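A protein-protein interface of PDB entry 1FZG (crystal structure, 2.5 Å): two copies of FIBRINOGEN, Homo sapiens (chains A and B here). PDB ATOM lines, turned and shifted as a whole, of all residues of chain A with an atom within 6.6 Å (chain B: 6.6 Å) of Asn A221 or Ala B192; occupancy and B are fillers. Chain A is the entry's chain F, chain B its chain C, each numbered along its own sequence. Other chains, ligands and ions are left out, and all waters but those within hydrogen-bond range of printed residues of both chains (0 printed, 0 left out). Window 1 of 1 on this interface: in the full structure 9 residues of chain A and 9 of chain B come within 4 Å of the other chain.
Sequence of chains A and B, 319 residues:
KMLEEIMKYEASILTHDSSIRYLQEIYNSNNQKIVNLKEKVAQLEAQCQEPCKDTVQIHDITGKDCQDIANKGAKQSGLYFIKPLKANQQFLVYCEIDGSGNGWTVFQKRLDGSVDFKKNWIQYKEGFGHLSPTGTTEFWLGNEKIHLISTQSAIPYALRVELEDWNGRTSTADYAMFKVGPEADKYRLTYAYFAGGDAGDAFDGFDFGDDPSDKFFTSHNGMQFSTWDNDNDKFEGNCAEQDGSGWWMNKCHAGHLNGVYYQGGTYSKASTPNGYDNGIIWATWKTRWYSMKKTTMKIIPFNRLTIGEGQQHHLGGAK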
ATOM      1  N   ARG A 188     -12.143  17.321  32.452  1.00  0.00           N
ATOM      2  CA  ARG A 188     -12.075  18.107  31.256  1.00  0.00           C
ATOM      3  C   ARG A 188     -12.132  19.604  31.607  1.00  0.00           C
ATOM      4  O   ARG A 188     -12.868  20.121  32.487  1.00  0.00           O
ATOM      5  CB  ARG A 188     -13.253  17.839  30.301  1.00  0.00           C
ATOM      6  CG  ARG A 188     -13.022  18.339  28.858  1.00  0.00           C
ATOM      7  CD  ARG A 188     -14.372  18.466  28.132  1.00  0.00           C
ATOM      8  NE  ARG A 188     -15.124  17.214  28.152  1.00  0.00           N
ATOM      9  CZ  ARG A 188     -14.834  16.270  27.250  1.00  0.00           C
ATOM     10  NH1 ARG A 188     -13.934  16.473  26.306  1.00  0.00           N
ATOM     11  NH2 ARG A 188     -15.478  15.124  27.343  1.00  0.00           N
ATOM     12  N   LEU A 189     -11.144  20.246  30.947  1.00  0.00           N
ATOM     13  CA  LEU A 189     -11.028  21.692  31.076  1.00  0.00           C
ATOM     14  C   LEU A 189     -11.927  22.455  30.099  1.00  0.00           C
ATOM     15  O   LEU A 189     -11.921  22.056  28.919  1.00  0.00           O
ATOM     16  CB  LEU A 189      -9.574  21.991  30.663  1.00  0.00           C
ATOM     17  CG  LEU A 189      -9.181  23.481  30.553  1.00  0.00           C
ATOM     18  CD1 LEU A 189      -9.336  24.092  31.922  1.00  0.00           C
ATOM     19  CD2 LEU A 189      -7.731  23.589  30.146  1.00  0.00           C
ATOM     20  N   THR A 190     -12.604  23.539  30.453  1.00  0.00           N
ATOM     21  CA  THR A 190     -13.274  24.260  29.349  1.00  0.00           C
ATOM     22  C   THR A 190     -13.334  25.719  29.715  1.00  0.00           C
ATOM     23  O   THR A 190     -13.447  25.969  30.914  1.00  0.00           O
ATOM     24  CB  THR A 190     -14.720  23.837  29.080  1.00  0.00           C
ATOM     25  OG1 THR A 190     -15.494  24.062  30.276  1.00  0.00           O
ATOM     26  CG2 THR A 190     -14.837  22.378  28.631  1.00  0.00           C
ATOM     27  N   TYR A 191     -13.198  26.644  28.796  1.00  0.00           N
ATOM     28  CA  TYR A 191     -13.330  28.076  29.072  1.00  0.00           C
ATOM     29  C   TYR A 191     -14.109  28.719  27.926  1.00  0.00           C
ATOM     30  O   TYR A 191     -14.211  28.146  26.838  1.00  0.00           O
ATOM     31  CB  TYR A 191     -11.965  28.737  29.304  1.00  0.00           C
ATOM     32  CG  TYR A 191     -10.999  28.549  28.162  1.00  0.00           C
ATOM     33  CD1 TYR A 191     -10.180  27.442  28.099  1.00  0.00           C
ATOM     34  CD2 TYR A 191     -10.939  29.483  27.115  1.00  0.00           C
ATOM     35  CE1 TYR A 191      -9.319  27.270  27.036  1.00  0.00           C
ATOM     36  CE2 TYR A 191     -10.069  29.305  26.068  1.00  0.00           C
ATOM     37  CZ  TYR A 191      -9.271  28.183  26.028  1.00  0.00           C
ATOM     38  OH  TYR A 191      -8.407  27.970  24.965  1.00  0.00           O
ATOM     39  N   ALA A 192     -14.807  29.832  28.131  1.00  0.00           N
ATOM     40  CA  ALA A 192     -15.564  30.474  27.061  1.00  0.00           C
ATOM     41  C   ALA A 192     -14.598  31.201  26.125  1.00  0.00           C
ATOM     42  O   ALA A 192     -14.716  30.953  24.918  1.00  0.00           O
ATOM     43  CB  ALA A 192     -16.582  31.440  27.591  1.00  0.00           C
ATOM     44  N   TYR A 193     -13.635  31.945  26.645  1.00  0.00           N
ATOM     45  CA  TYR A 193     -12.668  32.634  25.811  1.00  0.00           C
ATOM     46  C   TYR A 193     -11.460  33.188  26.545  1.00  0.00           C
ATOM     47  O   TYR A 193     -11.379  33.442  27.748  1.00  0.00           O
ATOM     48  CB  TYR A 193     -13.335  33.808  25.010  1.00  0.00           C
ATOM     49  CG  TYR A 193     -13.892  34.856  25.960  1.00  0.00           C
ATOM     50  CD1 TYR A 193     -15.165  34.744  26.499  1.00  0.00           C
ATOM     51  CD2 TYR A 193     -13.104  35.932  26.338  1.00  0.00           C
ATOM     52  CE1 TYR A 193     -15.665  35.691  27.358  1.00  0.00           C
ATOM     53  CE2 TYR A 193     -13.588  36.846  27.238  1.00  0.00           C
ATOM     54  CZ  TYR A 193     -14.853  36.735  27.730  1.00  0.00           C
ATOM     55  OH  TYR A 193     -15.263  37.703  28.640  1.00  0.00           O
ATOM     56  N   PHE A 203      -3.356  28.267  25.490  1.00  0.00           N
ATOM     57  CA  PHE A 203      -4.352  27.209  25.517  1.00  0.00           C
ATOM     58  C   PHE A 203      -4.985  27.104  24.136  1.00  0.00           C
ATOM     59  O   PHE A 203      -5.710  26.182  23.822  1.00  0.00           O
ATOM     60  CB  PHE A 203      -5.387  27.406  26.596  1.00  0.00           C
ATOM     61  CG  PHE A 203      -5.072  27.031  28.018  1.00  0.00           C
ATOM     62  CD1 PHE A 203      -4.008  26.181  28.343  1.00  0.00           C
ATOM     63  CD2 PHE A 203      -5.911  27.443  29.028  1.00  0.00           C
ATOM     64  CE1 PHE A 203      -3.786  25.824  29.640  1.00  0.00           C
ATOM     65  CE2 PHE A 203      -5.653  27.120  30.350  1.00  0.00           C
ATOM     66  CZ  PHE A 203      -4.600  26.277  30.688  1.00  0.00           C
ATOM     67  N   ASP A 204      -4.697  28.060  23.258  1.00  0.00           N
ATOM     68  CA  ASP A 204      -5.331  27.989  21.935  1.00  0.00           C
ATOM     69  C   ASP A 204      -4.524  27.088  21.023  1.00  0.00           C
ATOM     70  O   ASP A 204      -5.018  26.836  19.928  1.00  0.00           O
ATOM     71  CB  ASP A 204      -5.508  29.402  21.437  1.00  0.00           C
ATOM     72  CG  ASP A 204      -6.498  29.567  20.306  1.00  0.00           C
ATOM     73  OD1 ASP A 204      -7.698  29.277  20.393  1.00  0.00           O
ATOM     74  OD2 ASP A 204      -6.060  30.106  19.253  1.00  0.00           O
ATOM     75  N   SER A 219      -3.935  22.396  21.036  1.00  0.00           N
ATOM     76  CA  SER A 219      -4.804  23.287  21.838  1.00  0.00           C
ATOM     77  C   SER A 219      -5.302  22.601  23.110  1.00  0.00           C
ATOM     78  O   SER A 219      -5.292  21.369  23.184  1.00  0.00           O
ATOM     79  CB  SER A 219      -5.921  23.659  20.886  1.00  0.00           C
ATOM     80  OG  SER A 219      -6.643  22.470  20.607  1.00  0.00           O
ATOM     81  N   HIS A 220      -5.860  23.257  24.118  1.00  0.00           N
ATOM     82  CA  HIS A 220      -6.220  22.634  25.354  1.00  0.00           C
ATOM     83  C   HIS A 220      -7.693  22.732  25.684  1.00  0.00           C
ATOM     84  O   HIS A 220      -8.121  21.846  26.403  1.00  0.00           O
ATOM     85  CB  HIS A 220      -5.372  23.122  26.571  1.00  0.00           C
ATOM     86  CG  HIS A 220      -3.978  22.603  26.376  1.00  0.00           C
ATOM     87  ND1 HIS A 220      -2.974  23.361  25.786  1.00  0.00           N
ATOM     88  CD2 HIS A 220      -3.414  21.417  26.631  1.00  0.00           C
ATOM     89  CE1 HIS A 220      -1.841  22.663  25.695  1.00  0.00           C
ATOM     90  NE2 HIS A 220      -2.112  21.480  26.181  1.00  0.00           N
ATOM     91  N   ASN A 221      -8.368  23.770  25.246  1.00  0.00           N
ATOM     92  CA  ASN A 221      -9.748  24.009  25.559  1.00  0.00           C
ATOM     93  C   ASN A 221     -10.500  22.731  25.236  1.00  0.00           C
ATOM     94  O   ASN A 221     -10.274  22.158  24.181  1.00  0.00           O
ATOM     95  CB  ASN A 221     -10.275  25.213  24.741  1.00  0.00           C
ATOM     96  CG  ASN A 221     -11.550  25.750  25.371  1.00  0.00           C
ATOM     97  OD1 ASN A 221     -11.980  25.241  26.445  1.00  0.00           O
ATOM     98  ND2 ASN A 221     -12.145  26.764  24.798  1.00  0.00           N
ATOM     99  N   GLY A 222     -11.290  22.177  26.134  1.00  0.00           N
ATOM    100  CA  GLY A 222     -11.970  20.933  25.822  1.00  0.00           C
ATOM    101  C   GLY A 222     -11.278  19.638  26.079  1.00  0.00           C
ATOM    102  O   GLY A 222     -11.925  18.611  26.028  1.00  0.00           O
ATOM    103  N   MET A 223     -10.017  19.583  26.435  1.00  0.00           N
ATOM    104  CA  MET A 223      -9.279  18.370  26.685  1.00  0.00           C
ATOM    105  C   MET A 223      -9.614  17.750  28.030  1.00  0.00           C
ATOM    106  O   MET A 223      -9.944  18.389  29.024  1.00  0.00           O
ATOM    107  CB  MET A 223      -7.789  18.625  26.629  1.00  0.00           C
ATOM    108  CG  MET A 223      -7.185  18.958  25.275  1.00  0.00           C
ATOM    109  SD  MET A 223      -7.596  17.707  24.017  1.00  0.00           S
ATOM    110  CE  MET A 223      -8.946  18.496  23.249  1.00  0.00           C
ATOM    111  N   ASN A 250      -3.314  16.729  24.544  1.00  0.00           N
ATOM    112  CA  ASN A 250      -3.939  16.667  23.256  1.00  0.00           C
ATOM    113  C   ASN A 250      -2.820  16.405  22.295  1.00  0.00           C
ATOM    114  O   ASN A 250      -2.292  17.314  21.579  1.00  0.00           O
ATOM    115  CB  ASN A 250      -4.612  18.026  22.941  1.00  0.00           C
ATOM    116  CG  ASN A 250      -5.083  18.291  21.543  1.00  0.00           C
ATOM    117  OD1 ASN A 250      -4.927  17.463  20.675  1.00  0.00           O
ATOM    118  ND2 ASN A 250      -5.727  19.411  21.154  1.00  0.00           N
ATOM    119  N   TYR B 175     -22.155  23.852  19.791  1.00  0.00           N
ATOM    120  CA  TYR B 175     -20.744  23.545  19.886  1.00  0.00           C
ATOM    121  C   TYR B 175     -19.913  24.810  20.036  1.00  0.00           C
ATOM    122  O   TYR B 175     -20.120  25.785  19.274  1.00  0.00           O
ATOM    123  CB  TYR B 175     -20.416  22.905  18.501  1.00  0.00           C
ATOM    124  CG  TYR B 175     -21.058  21.537  18.468  1.00  0.00           C
ATOM    125  CD1 TYR B 175     -20.324  20.537  19.051  1.00  0.00           C
ATOM    126  CD2 TYR B 175     -22.298  21.235  17.936  1.00  0.00           C
ATOM    127  CE1 TYR B 175     -20.824  19.267  19.074  1.00  0.00           C
ATOM    128  CE2 TYR B 175     -22.813  19.942  17.974  1.00  0.00           C
ATOM    129  CZ  TYR B 175     -22.065  18.967  18.555  1.00  0.00           C
ATOM    130  OH  TYR B 175     -22.391  17.640  18.717  1.00  0.00           O
ATOM    131  N   ALA B 176     -18.949  24.817  20.967  1.00  0.00           N
ATOM    132  CA  ALA B 176     -18.220  26.056  21.203  1.00  0.00           C
ATOM    133  C   ALA B 176     -16.906  26.127  20.479  1.00  0.00           C
ATOM    134  O   ALA B 176     -16.245  25.091  20.327  1.00  0.00           O
ATOM    135  CB  ALA B 176     -18.020  26.215  22.704  1.00  0.00           C
ATOM    136  N   MET B 177     -16.485  27.354  20.205  1.00  0.00           N
ATOM    137  CA  MET B 177     -15.225  27.502  19.487  1.00  0.00           C
ATOM    138  C   MET B 177     -15.137  26.535  18.294  1.00  0.00           C
ATOM    139  O   MET B 177     -14.202  25.720  18.137  1.00  0.00           O
ATOM    140  CB  MET B 177     -14.016  27.338  20.406  1.00  0.00           C
ATOM    141  CG  MET B 177     -13.461  28.498  21.184  1.00  0.00           C
ATOM    142  SD  MET B 177     -14.506  28.906  22.617  1.00  0.00           S
ATOM    143  CE  MET B 177     -14.862  27.259  23.276  1.00  0.00           C
ATOM    144  N   PHE B 178     -16.074  26.661  17.376  1.00  0.00           N
ATOM    145  CA  PHE B 178     -16.244  25.930  16.161  1.00  0.00           C
ATOM    146  C   PHE B 178     -15.258  26.425  15.115  1.00  0.00           C
ATOM    147  O   PHE B 178     -15.268  27.642  14.875  1.00  0.00           O
ATOM    148  CB  PHE B 178     -17.653  26.155  15.571  1.00  0.00           C
ATOM    149  CG  PHE B 178     -17.786  25.611  14.161  1.00  0.00           C
ATOM    150  CD1 PHE B 178     -17.967  24.269  13.907  1.00  0.00           C
ATOM    151  CD2 PHE B 178     -17.713  26.473  13.068  1.00  0.00           C
ATOM    152  CE1 PHE B 178     -18.031  23.782  12.604  1.00  0.00           C
ATOM    153  CE2 PHE B 178     -17.823  25.996  11.778  1.00  0.00           C
ATOM    154  CZ  PHE B 178     -17.963  24.636  11.539  1.00  0.00           C
ATOM    155  N   THR B 190     -13.291  21.363  13.915  1.00  0.00           N
ATOM    156  CA  THR B 190     -12.866  21.313  15.307  1.00  0.00           C
ATOM    157  C   THR B 190     -13.731  22.198  16.180  1.00  0.00           C
ATOM    158  O   THR B 190     -14.084  23.250  15.634  1.00  0.00           O
ATOM    159  CB  THR B 190     -11.429  21.863  15.479  1.00  0.00           C
ATOM    160  OG1 THR B 190     -11.424  23.248  15.124  1.00  0.00           O
ATOM    161  CG2 THR B 190     -10.508  21.107  14.519  1.00  0.00           C
ATOM    162  N   TYR B 191     -14.053  21.751  17.360  1.00  0.00           N
ATOM    163  CA  TYR B 191     -14.777  22.589  18.286  1.00  0.00           C
ATOM    164  C   TYR B 191     -14.110  22.308  19.637  1.00  0.00           C
ATOM    165  O   TYR B 191     -13.250  21.401  19.662  1.00  0.00           O
ATOM    166  CB  TYR B 191     -16.253  22.306  18.314  1.00  0.00           C
ATOM    167  CG  TYR B 191     -16.554  20.859  18.517  1.00  0.00           C
ATOM    168  CD1 TYR B 191     -16.672  20.298  19.780  1.00  0.00           C
ATOM    169  CD2 TYR B 191     -16.643  20.013  17.399  1.00  0.00           C
ATOM    170  CE1 TYR B 191     -16.943  18.946  19.961  1.00  0.00           C
ATOM    171  CE2 TYR B 191     -16.878  18.658  17.570  1.00  0.00           C
ATOM    172  CZ  TYR B 191     -17.047  18.149  18.832  1.00  0.00           C
ATOM    173  OH  TYR B 191     -17.336  16.815  18.953  1.00  0.00           O
ATOM    174  N   ALA B 192     -14.430  23.063  20.693  1.00  0.00           N
ATOM    175  CA  ALA B 192     -13.707  22.787  21.945  1.00  0.00           C
ATOM    176  C   ALA B 192     -14.572  21.813  22.700  1.00  0.00           C
ATOM    177  O   ALA B 192     -14.241  20.780  23.208  1.00  0.00           O
ATOM    178  CB  ALA B 192     -13.572  24.062  22.763  1.00  0.00           C
ATOM    179  N   TYR B 193     -15.848  22.124  22.738  1.00  0.00           N
ATOM    180  CA  TYR B 193     -16.755  21.227  23.429  1.00  0.00           C
ATOM    181  C   TYR B 193     -18.167  21.463  22.980  1.00  0.00           C
ATOM    182  O   TYR B 193     -18.569  22.443  22.442  1.00  0.00           O
ATOM    183  CB  TYR B 193     -16.576  21.495  24.936  1.00  0.00           C
ATOM    184  CG  TYR B 193     -16.819  22.908  25.378  1.00  0.00           C
ATOM    185  CD1 TYR B 193     -18.065  23.382  25.778  1.00  0.00           C
ATOM    186  CD2 TYR B 193     -15.716  23.766  25.412  1.00  0.00           C
ATOM    187  CE1 TYR B 193     -18.242  24.713  26.186  1.00  0.00           C
ATOM    188  CE2 TYR B 193     -15.855  25.084  25.850  1.00  0.00           C
ATOM    189  CZ  TYR B 193     -17.124  25.518  26.208  1.00  0.00           C
ATOM    190  OH  TYR B 193     -17.135  26.844  26.560  1.00  0.00           O
ATOM    191  N   PHE B 194     -19.030  20.549  23.269  1.00  0.00           N
ATOM    192  CA  PHE B 194     -20.458  20.549  23.131  1.00  0.00           C
ATOM    193  C   PHE B 194     -20.991  21.524  24.171  1.00  0.00           C
ATOM    194  O   PHE B 194     -20.659  21.375  25.343  1.00  0.00           O
ATOM    195  CB  PHE B 194     -20.900  19.084  23.391  1.00  0.00           C
ATOM    196  CG  PHE B 194     -22.417  18.975  23.424  1.00  0.00           C
ATOM    197  CD1 PHE B 194     -23.134  19.296  22.284  1.00  0.00           C
ATOM    198  CD2 PHE B 194     -23.083  18.563  24.552  1.00  0.00           C
ATOM    199  CE1 PHE B 194     -24.507  19.239  22.291  1.00  0.00           C
ATOM    200  CE2 PHE B 194     -24.453  18.477  24.550  1.00  0.00           C
ATOM    201  CZ  PHE B 194     -25.187  18.819  23.403  1.00  0.00           C
ATOM    202  N   ASN B 221     -15.132  15.277  15.923  1.00  0.00           N
ATOM    203  CA  ASN B 221     -14.177  16.358  16.257  1.00  0.00           C
ATOM    204  C   ASN B 221     -12.826  15.999  15.730  1.00  0.00           C
ATOM    205  O   ASN B 221     -12.471  14.811  15.760  1.00  0.00           O
ATOM    206  CB  ASN B 221     -14.250  16.493  17.774  1.00  0.00           C
ATOM    207  CG  ASN B 221     -13.702  17.845  18.170  1.00  0.00           C
ATOM    208  OD1 ASN B 221     -13.315  18.660  17.344  1.00  0.00           O
ATOM    209  ND2 ASN B 221     -13.719  18.018  19.454  1.00  0.00           N
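The side-chain hydroxyl (OH) of Tyr B193 lies within hydrogen-bond range of the backbone carbonyl oxygen (O) of Tyr A191 (3.2 Å). SD of Met B177 sits close to O of Ala A192, at 3.1 Å.
NH1 of Arg A188 sits at hydrogen-bond distance from O of Gly A222 (2.9 Å). The backbone carbonyl oxygen of Leu A189 sits at hydrogen-bond distance from the backbone NH of Gly A222, 2.9 Å away. The backbone NH of Tyr A191 sits at hydrogen-bond distance from the side-chain amide oxygen of Asn A221, 3.0 Å away. The side-chain hydroxyl of Tyr A191 is in hydrogen-bond range of the backbone carbonyl oxygen of Phe A203, 3.4 Å away. O of Tyr B193 sits at hydrogen-bond distance from N of Ala B176, 2.8 Å away. The backbone NH (N) of Ala B192 sits at hydrogen-bond distance from the backbone carbonyl oxygen (O) of Ala B176.
Thr A190 touches Tyr B193. Tyr A191 touches Met B177 (O to CE, 3.7 Å). CA of Ala A192 touches OH of Tyr B193 (3.99 Å). CE of Met B177 touches ND2 of Asn A221, at 3.2 Å. Ala B192 touches Asn A221 (CB to ND2, 3.7 Å). Asn A221 touches Tyr B193. Gly A222 touches Ala B192.
Of chain B, only Met B177, Ala B192 and Tyr B193 come within 4 Å of Asn A221. Of chain A, only Asn A221 and Gly A222 come within 4 Å of Ala B192. Printed residues of chain A within 4 Å of Tyr B193: Thr A190, Tyr A191, Ala A192 and Asn A221. Of the printed residues of chain A, Met B177 touches Tyr A191, Ala A192 and Asn A221. Of the printed residues of chain B, Gly A222 touches Ala B192 (3.5 Å). Of the printed residues of chain B, Tyr A191 touches Met B177 (3.7 Å) and Tyr B193 (3.2 Å). Printed residues of chain B within 4 Å of Thr A190: Tyr B193 (3.6 Å). The nearest residue of chain B that does not touch Asn A221 is Tyr B191 (5.5 Å). The nearest residue of chain A that does not touch Ala B192 is Arg A188 (5.3 Å). The nearest printed residue of chain A that does not touch Tyr B193 is Gly A222 (4.7 Å).
Of the 10 printed residues of chain B, 3 touch a printed residue of chain A. Hydrophobic or aromatic side chains of chain B that line the printed part of chain A: Met B177, Ala B192 and Tyr B193. Along chain B the printed residues that touch a printed residue of chain A span positions 177 to 193. Among the printed residues, no Asp or Glu carboxylate lies within 4 Å of a Lys or Arg side-chain nitrogen of the other chain.
Thr A190 touches Tyr B193, but with the chains exchanged Tyr A193 does not touch Thr B190 (13.9 Å). Tyr A191 touches Tyr B193, but with the chains exchanged Tyr A193 does not touch Tyr B191 (11.9 Å). Ala A192 touches Tyr B193, but with the chains exchanged Tyr A193 does not touch Ala B192 (8.8 Å). Asn A221 touches Ala B192, but with the chains exchanged Ala A192 does not touch Asn B221 (14.1 Å). 5 positions are printed for both chains. Of the 9 pairs that touch across the chains among the printed residues, none has its exchanged pair printed and touching as well.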
